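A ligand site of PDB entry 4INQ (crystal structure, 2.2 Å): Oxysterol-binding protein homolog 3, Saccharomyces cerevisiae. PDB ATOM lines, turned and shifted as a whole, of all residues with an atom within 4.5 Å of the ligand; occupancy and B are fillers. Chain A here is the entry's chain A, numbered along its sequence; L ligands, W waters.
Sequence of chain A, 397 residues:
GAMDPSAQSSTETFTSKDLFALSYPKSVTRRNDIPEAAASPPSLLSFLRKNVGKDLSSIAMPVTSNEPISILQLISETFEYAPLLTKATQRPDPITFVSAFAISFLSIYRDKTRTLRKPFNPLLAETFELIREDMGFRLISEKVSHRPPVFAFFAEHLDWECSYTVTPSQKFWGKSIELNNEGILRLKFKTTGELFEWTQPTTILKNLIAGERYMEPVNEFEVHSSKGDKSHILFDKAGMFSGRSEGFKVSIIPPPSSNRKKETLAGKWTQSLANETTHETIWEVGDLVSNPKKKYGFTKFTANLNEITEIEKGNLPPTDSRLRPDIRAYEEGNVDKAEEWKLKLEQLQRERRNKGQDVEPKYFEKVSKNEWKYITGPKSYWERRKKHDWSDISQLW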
ATOM      1  N   LEU A  44      15.151   5.700   1.884  1.00  0.00           N
ATOM      2  CA  LEU A  44      14.709   5.899   0.517  1.00  0.00           C
ATOM      3  C   LEU A  44      14.030   7.269   0.388  1.00  0.00           C
ATOM      4  O   LEU A  44      14.308   8.017  -0.550  1.00  0.00           O
ATOM      5  CB  LEU A  44      13.756   4.765   0.134  1.00  0.00           C
ATOM      6  CG  LEU A  44      13.039   4.774  -1.222  1.00  0.00           C
ATOM      7  CD1 LEU A  44      11.839   5.690  -1.156  1.00  0.00           C
ATOM      8  CD2 LEU A  44      14.003   5.194  -2.325  1.00  0.00           C
ATOM      9  N   LEU A  56      13.758  11.940 -10.511  1.00  0.00           N
ATOM     10  CA  LEU A  56      14.578  10.735 -10.491  1.00  0.00           C
ATOM     11  C   LEU A  56      14.876   9.964 -11.772  1.00  0.00           C
ATOM     12  O   LEU A  56      15.067  10.535 -12.849  1.00  0.00           O
ATOM     13  CB  LEU A  56      13.979   9.772  -9.459  1.00  0.00           C
ATOM     14  CG  LEU A  56      12.447   9.673  -9.513  1.00  0.00           C
ATOM     15  CD1 LEU A  56      12.034   8.958 -10.792  1.00  0.00           C
ATOM     16  CD2 LEU A  56      11.924   8.928  -8.294  1.00  0.00           C
ATOM     17  N   SER A  57      14.952   8.645 -11.616  1.00  0.00           N
ATOM     18  CA  SER A  57      15.240   7.697 -12.690  1.00  0.00           C
ATOM     19  C   SER A  57      16.741   7.592 -12.936  1.00  0.00           C
ATOM     20  O   SER A  57      17.434   6.803 -12.284  1.00  0.00           O
ATOM     21  CB  SER A  57      14.540   8.093 -13.991  1.00  0.00           C
ATOM     22  OG  SER A  57      14.899   7.223 -15.053  1.00  0.00           O
ATOM     23  N   SER A  58      17.236   8.405 -13.855  1.00  0.00           N
ATOM     24  CA  SER A  58      18.655   8.406 -14.194  1.00  0.00           C
ATOM     25  C   SER A  58      19.475   9.147 -13.133  1.00  0.00           C
ATOM     26  O   SER A  58      20.395   9.900 -13.453  1.00  0.00           O
ATOM     27  CB  SER A  58      18.868   9.055 -15.561  1.00  0.00           C
ATOM     28  OG  SER A  58      20.183   8.823 -16.044  1.00  0.00           O
ATOM     29  N   ILE A  59      19.119   8.921 -11.869  1.00  0.00           N
ATOM     30  CA  ILE A  59      19.818   9.523 -10.738  1.00  0.00           C
ATOM     31  C   ILE A  59      20.442   8.404  -9.915  1.00  0.00           C
ATOM     32  O   ILE A  59      19.730   7.528  -9.399  1.00  0.00           O
ATOM     33  CB  ILE A  59      18.843  10.310  -9.828  1.00  0.00           C
ATOM     34  CG1 ILE A  59      18.070  11.343 -10.649  1.00  0.00           C
ATOM     35  CG2 ILE A  59      19.614  11.007  -8.722  1.00  0.00           C
ATOM     36  CD1 ILE A  59      18.952  12.343 -11.391  1.00  0.00           C
ATOM     37  N   ALA A  60      21.767   8.420  -9.796  1.00  0.00           N
ATOM     38  CA  ALA A  60      22.490   7.388  -9.064  1.00  0.00           C
ATOM     39  C   ALA A  60      22.183   7.346  -7.567  1.00  0.00           C
ATOM     40  O   ALA A  60      21.719   8.338  -6.997  1.00  0.00           O
ATOM     41  CB  ALA A  60      23.988   7.578  -9.258  1.00  0.00           C
ATOM     42  N   MET A  61      22.438   6.190  -6.971  1.00  0.00           N
ATOM     43  CA  MET A  61      22.223   5.958  -5.540  1.00  0.00           C
ATOM     44  C   MET A  61      23.442   5.214  -5.014  1.00  0.00           C
ATOM     45  O   MET A  61      24.102   4.495  -5.761  1.00  0.00           O
ATOM     46  CB  MET A  61      20.979   5.098  -5.307  1.00  0.00           C
ATOM     47  CG  MET A  61      19.652   5.774  -5.664  1.00  0.00           C
ATOM     48  SD  MET A  61      18.220   4.768  -5.210  1.00  0.00           S
ATOM     49  CE  MET A  61      18.243   4.927  -3.444  1.00  0.00           C
ATOM     50  N   ASN A  66      21.726  -1.074  -2.076  1.00  0.00           N
ATOM     51  CA  ASN A  66      21.522  -2.336  -2.772  1.00  0.00           C
ATOM     52  C   ASN A  66      21.640  -3.588  -1.904  1.00  0.00           C
ATOM     53  O   ASN A  66      22.149  -3.555  -0.788  1.00  0.00           O
ATOM     54  CB  ASN A  66      22.545  -2.480  -3.911  1.00  0.00           C
ATOM     55  CG  ASN A  66      22.345  -1.464  -5.041  1.00  0.00           C
ATOM     56  OD1 ASN A  66      23.252  -1.223  -5.832  1.00  0.00           O
ATOM     57  ND2 ASN A  66      21.155  -0.896  -5.141  1.00  0.00           N
ATOM     58  N   ILE A  71      18.946  -6.909 -10.774  1.00  0.00           N
ATOM     59  CA  ILE A  71      17.516  -6.986 -11.049  1.00  0.00           C
ATOM     60  C   ILE A  71      17.196  -8.238 -11.861  1.00  0.00           C
ATOM     61  O   ILE A  71      16.135  -8.836 -11.705  1.00  0.00           O
ATOM     62  CB  ILE A  71      17.024  -5.763 -11.857  1.00  0.00           C
ATOM     63  CG1 ILE A  71      17.060  -4.508 -10.982  1.00  0.00           C
ATOM     64  CG2 ILE A  71      15.614  -5.998 -12.351  1.00  0.00           C
ATOM     65  CD1 ILE A  71      16.828  -3.239 -11.780  1.00  0.00           C
ATOM     66  N   LEU A  74      16.783 -10.879  -9.379  1.00  0.00           N
ATOM     67  CA  LEU A  74      15.559 -10.683  -8.603  1.00  0.00           C
ATOM     68  C   LEU A  74      14.343 -11.230  -9.379  1.00  0.00           C
ATOM     69  O   LEU A  74      13.543 -12.016  -8.854  1.00  0.00           O
ATOM     70  CB  LEU A  74      15.331  -9.202  -8.327  1.00  0.00           C
ATOM     71  CG  LEU A  74      13.925  -8.879  -7.823  1.00  0.00           C
ATOM     72  CD1 LEU A  74      13.814  -9.190  -6.336  1.00  0.00           C
ATOM     73  CD2 LEU A  74      13.599  -7.416  -8.078  1.00  0.00           C
ATOM     74  N   LYS A 118      17.441  -2.502  -2.636  1.00  0.00           N
ATOM     75  CA  LYS A 118      17.088  -2.868  -4.009  1.00  0.00           C
ATOM     76  C   LYS A 118      18.218  -3.625  -4.705  1.00  0.00           C
ATOM     77  O   LYS A 118      19.376  -3.587  -4.251  1.00  0.00           O
ATOM     78  CB  LYS A 118      16.749  -1.623  -4.824  1.00  0.00           C
ATOM     79  CG  LYS A 118      17.964  -0.768  -5.147  1.00  0.00           C
ATOM     80  CD  LYS A 118      17.586   0.444  -5.965  1.00  0.00           C
ATOM     81  CE  LYS A 118      18.812   1.152  -6.488  1.00  0.00           C
ATOM     82  NZ  LYS A 118      19.576   0.248  -7.406  1.00  0.00           N
ATOM     83  N   PRO A 119      17.917  -4.304  -5.826  1.00  0.00           N
ATOM     84  CA  PRO A 119      18.957  -5.045  -6.534  1.00  0.00           C
ATOM     85  C   PRO A 119      19.881  -4.065  -7.248  1.00  0.00           C
ATOM     86  O   PRO A 119      19.530  -2.889  -7.401  1.00  0.00           O
ATOM     87  CB  PRO A 119      18.166  -5.880  -7.546  1.00  0.00           C
ATOM     88  CG  PRO A 119      16.768  -5.903  -6.994  1.00  0.00           C
ATOM     89  CD  PRO A 119      16.596  -4.538  -6.434  1.00  0.00           C
ATOM     90  N   ASN A 121      21.437  -2.321 -10.404  1.00  0.00           N
ATOM     91  CA  ASN A 121      20.878  -2.099 -11.718  1.00  0.00           C
ATOM     92  C   ASN A 121      21.836  -2.753 -12.695  1.00  0.00           C
ATOM     93  O   ASN A 121      23.037  -2.495 -12.655  1.00  0.00           O
ATOM     94  CB  ASN A 121      20.778  -0.600 -12.010  1.00  0.00           C
ATOM     95  CG  ASN A 121      19.364  -0.169 -12.381  1.00  0.00           C
ATOM     96  OD1 ASN A 121      18.775  -0.683 -13.341  1.00  0.00           O
ATOM     97  ND2 ASN A 121      18.817   0.776 -11.627  1.00  0.00           N
ATOM     98  N   HIS A 146      18.576   0.180 -21.800  1.00  0.00           N
ATOM     99  CA  HIS A 146      18.955   0.919 -20.605  1.00  0.00           C
ATOM    100  C   HIS A 146      17.948   2.009 -20.287  1.00  0.00           C
ATOM    101  O   HIS A 146      17.589   2.215 -19.121  1.00  0.00           O
ATOM    102  CB  HIS A 146      20.337   1.554 -20.800  1.00  0.00           C
ATOM    103  CG  HIS A 146      20.875   2.211 -19.563  1.00  0.00           C
ATOM    104  ND1 HIS A 146      21.298   3.527 -19.548  1.00  0.00           N
ATOM    105  CD2 HIS A 146      21.084   1.728 -18.317  1.00  0.00           C
ATOM    106  CE1 HIS A 146      21.747   3.818 -18.337  1.00  0.00           C
ATOM    107  NE2 HIS A 146      21.623   2.750 -17.575  1.00  0.00           N
ATOM    108  N   ARG A 147      17.482   2.720 -21.311  1.00  0.00           N
ATOM    109  CA  ARG A 147      16.520   3.794 -21.134  1.00  0.00           C
ATOM    110  C   ARG A 147      15.427   3.730 -22.195  1.00  0.00           C
ATOM    111  O   ARG A 147      15.657   4.021 -23.358  1.00  0.00           O
ATOM    112  CB  ARG A 147      17.238   5.148 -21.202  1.00  0.00           C
ATOM    113  CG  ARG A 147      18.379   5.278 -20.203  1.00  0.00           C
ATOM    114  CD  ARG A 147      17.878   5.816 -18.873  1.00  0.00           C
ATOM    115  NE  ARG A 147      17.874   7.284 -18.878  1.00  0.00           N
ATOM    116  CZ  ARG A 147      18.975   8.026 -18.834  1.00  0.00           C
ATOM    117  NH1 ARG A 147      20.164   7.458 -18.771  1.00  0.00           N
ATOM    118  NH2 ARG A 147      18.873   9.348 -18.857  1.00  0.00           N
ATOM    119  N   PRO A 168      10.542  -2.629 -14.965  1.00  0.00           N
ATOM    120  CA  PRO A 168      10.120  -2.262 -13.609  1.00  0.00           C
ATOM    121  C   PRO A 168       9.921  -0.755 -13.525  1.00  0.00           C
ATOM    122  O   PRO A 168      10.789   0.010 -13.941  1.00  0.00           O
ATOM    123  CB  PRO A 168      11.293  -2.735 -12.748  1.00  0.00           C
ATOM    124  CG  PRO A 168      11.876  -3.867 -13.553  1.00  0.00           C
ATOM    125  CD  PRO A 168      11.848  -3.312 -14.939  1.00  0.00           C
ATOM    126  N   GLN A 170       8.498   2.569 -10.945  1.00  0.00           N
ATOM    127  CA  GLN A 170       8.152   3.013  -9.590  1.00  0.00           C
ATOM    128  C   GLN A 170       7.588   4.426  -9.641  1.00  0.00           C
ATOM    129  O   GLN A 170       8.035   5.259 -10.435  1.00  0.00           O
ATOM    130  CB  GLN A 170       9.398   2.988  -8.696  1.00  0.00           C
ATOM    131  CG  GLN A 170      10.223   1.724  -8.799  1.00  0.00           C
ATOM    132  CD  GLN A 170      11.081   1.680 -10.041  1.00  0.00           C
ATOM    133  OE1 GLN A 170      11.290   0.613 -10.626  1.00  0.00           O
ATOM    134  NE2 GLN A 170      11.612   2.831 -10.455  1.00  0.00           N
ATOM    135  N   LEU A 179       4.904   0.075  -7.064  1.00  0.00           N
ATOM    136  CA  LEU A 179       5.850  -0.784  -7.775  1.00  0.00           C
ATOM    137  C   LEU A 179       5.112  -1.661  -8.771  1.00  0.00           C
ATOM    138  O   LEU A 179       4.207  -2.414  -8.418  1.00  0.00           O
ATOM    139  CB  LEU A 179       6.611  -1.671  -6.791  1.00  0.00           C
ATOM    140  CG  LEU A 179       7.460  -0.937  -5.759  1.00  0.00           C
ATOM    141  CD1 LEU A 179       7.990  -1.935  -4.746  1.00  0.00           C
ATOM    142  CD2 LEU A 179       8.596  -0.209  -6.449  1.00  0.00           C
ATOM    143  N   ASN A 181       5.756  -4.145 -12.397  1.00  0.00           N
ATOM    144  CA  ASN A 181       6.625  -4.737 -13.395  1.00  0.00           C
ATOM    145  C   ASN A 181       5.770  -4.645 -14.647  1.00  0.00           C
ATOM    146  O   ASN A 181       4.776  -5.359 -14.792  1.00  0.00           O
ATOM    147  CB  ASN A 181       6.933  -6.193 -13.064  1.00  0.00           C
ATOM    148  CG  ASN A 181       8.235  -6.355 -12.276  1.00  0.00           C
ATOM    149  OD1 ASN A 181       8.596  -7.460 -11.885  1.00  0.00           O
ATOM    150  ND2 ASN A 181       8.937  -5.252 -12.055  1.00  0.00           N
ATOM    151  N   LYS A 342      31.092   0.102  -8.375  1.00  0.00           N
ATOM    152  CA  LYS A 342      29.798   0.520  -8.909  1.00  0.00           C
ATOM    153  C   LYS A 342      29.974   1.793  -9.734  1.00  0.00           C
ATOM    154  O   LYS A 342      29.401   1.908 -10.814  1.00  0.00           O
ATOM    155  CB  LYS A 342      28.793   0.738  -7.766  1.00  0.00           C
ATOM    156  CG  LYS A 342      27.488   1.418  -8.183  1.00  0.00           C
ATOM    157  CD  LYS A 342      26.395   1.176  -7.137  1.00  0.00           C
ATOM    158  CE  LYS A 342      25.371   2.293  -7.075  1.00  0.00           C
ATOM    159  NZ  LYS A 342      24.617   2.524  -8.330  1.00  0.00           N
ATOM    160  N   GLU A 346      29.386   2.002 -13.971  1.00  0.00           N
ATOM    161  CA  GLU A 346      28.440   2.947 -14.553  1.00  0.00           C
ATOM    162  C   GLU A 346      29.130   3.994 -15.405  1.00  0.00           C
ATOM    163  O   GLU A 346      28.623   4.384 -16.449  1.00  0.00           O
ATOM    164  CB  GLU A 346      27.611   3.573 -13.426  1.00  0.00           C
ATOM    165  CG  GLU A 346      26.929   2.496 -12.594  1.00  0.00           C
ATOM    166  CD  GLU A 346      26.189   3.020 -11.379  1.00  0.00           C
ATOM    167  OE1 GLU A 346      26.719   3.916 -10.681  1.00  0.00           O
ATOM    168  OE2 GLU A 346      25.079   2.518 -11.114  1.00  0.00           O
ATOM    169  N   GLN A 349      30.027   2.386 -18.762  1.00  0.00           N
ATOM    170  CA  GLN A 349      28.860   2.211 -19.620  1.00  0.00           C
ATOM    171  C   GLN A 349      28.498   3.563 -20.216  1.00  0.00           C
ATOM    172  O   GLN A 349      28.049   3.678 -21.355  1.00  0.00           O
ATOM    173  CB  GLN A 349      27.684   1.665 -18.799  1.00  0.00           C
ATOM    174  CG  GLN A 349      26.334   1.779 -19.475  1.00  0.00           C
ATOM    175  CD  GLN A 349      25.272   0.960 -18.790  1.00  0.00           C
ATOM    176  OE1 GLN A 349      25.038  -0.188 -19.144  1.00  0.00           O
ATOM    177  NE2 GLN A 349      24.632   1.530 -17.776  1.00  0.00           N
ATOM    178  N   ARG A 350      28.709   4.596 -19.416  1.00  0.00           N
ATOM    179  CA  ARG A 350      28.427   5.951 -19.833  1.00  0.00           C
ATOM    180  C   ARG A 350      29.335   6.321 -21.011  1.00  0.00           C
ATOM    181  O   ARG A 350      28.851   6.773 -22.057  1.00  0.00           O
ATOM    182  CB  ARG A 350      28.660   6.882 -18.649  1.00  0.00           C
ATOM    183  CG  ARG A 350      27.788   8.095 -18.610  1.00  0.00           C
ATOM    184  CD  ARG A 350      27.775   8.617 -17.188  1.00  0.00           C
ATOM    185  NE  ARG A 350      27.057   7.716 -16.296  1.00  0.00           N
ATOM    186  CZ  ARG A 350      27.367   7.517 -15.019  1.00  0.00           C
ATOM    187  NH1 ARG A 350      28.398   8.163 -14.491  1.00  0.00           N
ATOM    188  NH2 ARG A 350      26.638   6.713 -14.258  1.00  0.00           N
HETATM  189  C1  LIG L   1      22.352   3.641 -11.846  1.00  0.00           C
HETATM  190  O1  LIG L   1      21.569   2.818 -10.967  1.00  0.00           O
HETATM  191  P1  LIG L   1      21.066   3.241  -9.503  1.00  0.00           P
HETATM  192  C2  LIG L   1      21.576   4.962 -12.216  1.00  0.00           C
HETATM  193  O2  LIG L   1      20.333   4.626 -12.872  1.00  0.00           O
HETATM  194  C3  LIG L   1      22.483   5.814 -13.162  1.00  0.00           C
HETATM  195  O3  LIG L   1      21.820   7.032 -13.526  1.00  0.00           O
HETATM  196  C4  LIG L   1      22.834   5.023 -14.456  1.00  0.00           C
HETATM  197  O4  LIG L   1      23.698   5.786 -15.286  1.00  0.00           O
HETATM  198  P2  LIG L   1      23.239   6.802 -16.434  1.00  0.00           P
HETATM  199  C5  LIG L   1      23.543   3.717 -14.091  1.00  0.00           C
HETATM  200  O5  LIG L   1      23.845   3.005 -15.276  1.00  0.00           O
HETATM  201  C6  LIG L   1      22.670   2.852 -13.157  1.00  0.00           C
HETATM  202  O6  LIG L   1      23.373   1.655 -12.870  1.00  0.00           O
HETATM  203  C7  LIG L   1      18.597   4.397  -9.163  1.00  0.00           C
HETATM  204  C8  LIG L   1      17.083   4.054  -9.398  1.00  0.00           C
HETATM  205  C9  LIG L   1      16.697   2.642  -8.934  1.00  0.00           C
HETATM  206  C10 LIG L   1      14.974   1.154  -9.633  1.00  0.00           C
HETATM  207  C11 LIG L   1      14.361   0.150  -8.620  1.00  0.00           C
HETATM  208  O7  LIG L   1      21.752   4.406  -8.905  1.00  0.00           O
HETATM  209  C12 LIG L   1      14.057  -1.211  -9.255  1.00  0.00           C
HETATM  210  O8  LIG L   1      21.236   1.924  -8.589  1.00  0.00           O
HETATM  211  C13 LIG L   1      13.329  -2.140  -8.277  1.00  0.00           C
HETATM  212  O9  LIG L   1      19.443   3.332  -9.581  1.00  0.00           O
HETATM  213  C14 LIG L   1      12.872  -3.432  -8.959  1.00  0.00           C
HETATM  214  O10 LIG L   1      16.295   5.136  -8.741  1.00  0.00           O
HETATM  215  C15 LIG L   1      11.760  -4.126  -8.174  1.00  0.00           C
HETATM  216  O11 LIG L   1      15.298   2.426  -9.205  1.00  0.00           O
HETATM  217  C16 LIG L   1      10.773  -4.881  -9.077  1.00  0.00           C
HETATM  218  O12 LIG L   1      15.164   0.799 -10.808  1.00  0.00           O
HETATM  219  C17 LIG L   1       9.303  -4.470  -8.821  1.00  0.00           C
HETATM  220  O13 LIG L   1      14.782   5.548 -10.402  1.00  0.00           O
HETATM  221  C18 LIG L   1      15.044   5.535  -9.210  1.00  0.00           C
HETATM  222  C19 LIG L   1      13.952   5.958  -8.230  1.00  0.00           C
HETATM  223  C20 LIG L   1      13.002   4.802  -7.925  1.00  0.00           C
HETATM  224  C21 LIG L   1      13.071   4.378  -6.457  1.00  0.00           C
HETATM  225  C22 LIG L   1      12.454   3.155  -6.206  1.00  0.00           C
HETATM  226  C23 LIG L   1      13.009   2.107  -5.443  1.00  0.00           C
HETATM  227  C24 LIG L   1      12.423   0.841  -5.234  1.00  0.00           C
HETATM  228  C25 LIG L   1      13.176   0.128  -4.286  1.00  0.00           C
HETATM  229  O14 LIG L   1      24.168   6.569 -17.710  1.00  0.00           O
HETATM  230  O15 LIG L   1      23.326   8.202 -15.894  1.00  0.00           O
HETATM  231  O16 LIG L   1      21.745   6.374 -16.905  1.00  0.00           O
HETATM  232  O   HOH W   1       6.508  -5.623  -7.773  1.00  0.00           O
HETATM  233  O   HOH W   2      23.029  -0.257  -8.783  1.00  0.00           O
HETATM  234  O   HOH W   3      14.735   0.786  -1.581  1.00  0.00           O
HETATM  235  O   HOH W   4      24.695  -0.691 -11.318  1.00  0.00           O
HETATM  236  O   HOH W   5      25.906   4.325 -16.841  1.00  0.00           O
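OE2 of Glu 346 is in hydrogen-bond range of O6 of the ligand, at 2.6 Å.
NZ of Lys 118 is in salt-bridge range of O8 of the ligand (2.6 Å).
The guanidinium group (NH1) of Arg 147 lies within salt-bridge range of an oxygen (O16) of the ligand (2.7 Å).
O7 of the ligand is in hydrogen-bond range of N of Met 61, at 2.7 Å.
NE2 of His 146 is in hydrogen-bond range of O5 of the ligand (3.2 Å).
The side-chain amide nitrogen of Gln 349 sits at hydrogen-bond distance from an oxygen (O5) of the ligand, at 3.0 Å.
O of Ser 58 sits close to O3 of the ligand (3.2 Å).
The side-chain hydroxyl (OG) of Ser 58 lies within hydrogen-bond range of an oxygen (O16) of the ligand (3.0 Å).
The backbone NH (N) of Ser 57 lies close to an oxygen (O13) of the ligand, 3.3 Å away.
NE of Arg 350 lies within salt-bridge range of O14 of the ligand (3.4 Å).
An oxygen (O9) of the ligand sits at hydrogen-bond distance from the side-chain amide nitrogen (ND2) of Asn 121.
The side-chain amino group (NZ) of Lys 342 lies within salt-bridge range of an oxygen (O8) of the ligand, 3.4 Å away.
The side-chain carboxylate of Glu 346 is in salt-bridge range of the side-chain amino group of Lys 342 (2.8 Å).
ND2 of Asn 66 sits close to NZ of Lys 118, 3.0 Å away.
NH1 of Arg 147 is in hydrogen-bond range of OG of Ser 58 (3.0 Å).
The backbone carbonyl oxygen (O) of Met 61 lies close to the side-chain amino group (NZ) of Lys 342 (3.3 Å).
A ring nitrogen (NE2) of His 146 sits at hydrogen-bond distance from the side-chain amide nitrogen (NE2) of Gln 349 (3.3 Å).
The backbone carbonyl oxygen (O) of Pro 168 lies close to the side-chain amide oxygen (OE1) of Gln 170, at 3.4 Å.
CD2 of Leu 56 touches C19 of the ligand (3.6 Å).
Ile 59 touches the ligand (O to C7, 3.3 Å).
CA of Ala 60 touches O7 of the ligand, at 3.1 Å.
Leu 74 touches the ligand (CD2 to C15, 3.8 Å).
Gln 170 touches the ligand.
ND2 of Asn 181 touches C17 of the ligand (3.3 Å).
Of the 23 residues printed, 17 come within 4 Å of the ligand.
Along chain A the residues within 4 Å of the ligand span positions 56 to 350.
The nearest printed residue that does not touch the ligand is Leu 179 (4.2 Å).
Water W2 lies within hydrogen-bond range of an oxygen (O8) of the ligand (2.8 Å), the backbone NH (N) of Asn 121 (3.1 Å), the side-chain amide oxygen (OD1) of Asn 66 (3.1 Å) and the side-chain amino group (NZ) of Lys 342 (3.2 Å).
Water W5 lies within hydrogen-bond range of O of Glu 346 (2.7 Å), O5 of the ligand (2.9 Å) and NE2 of Gln 349 (3.2 Å).
Water W4 lies within hydrogen-bond range of O of Asn 121 (2.8 Å), O6 of the ligand (3.1 Å) and OE2 of Glu 346 (3.2 Å).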
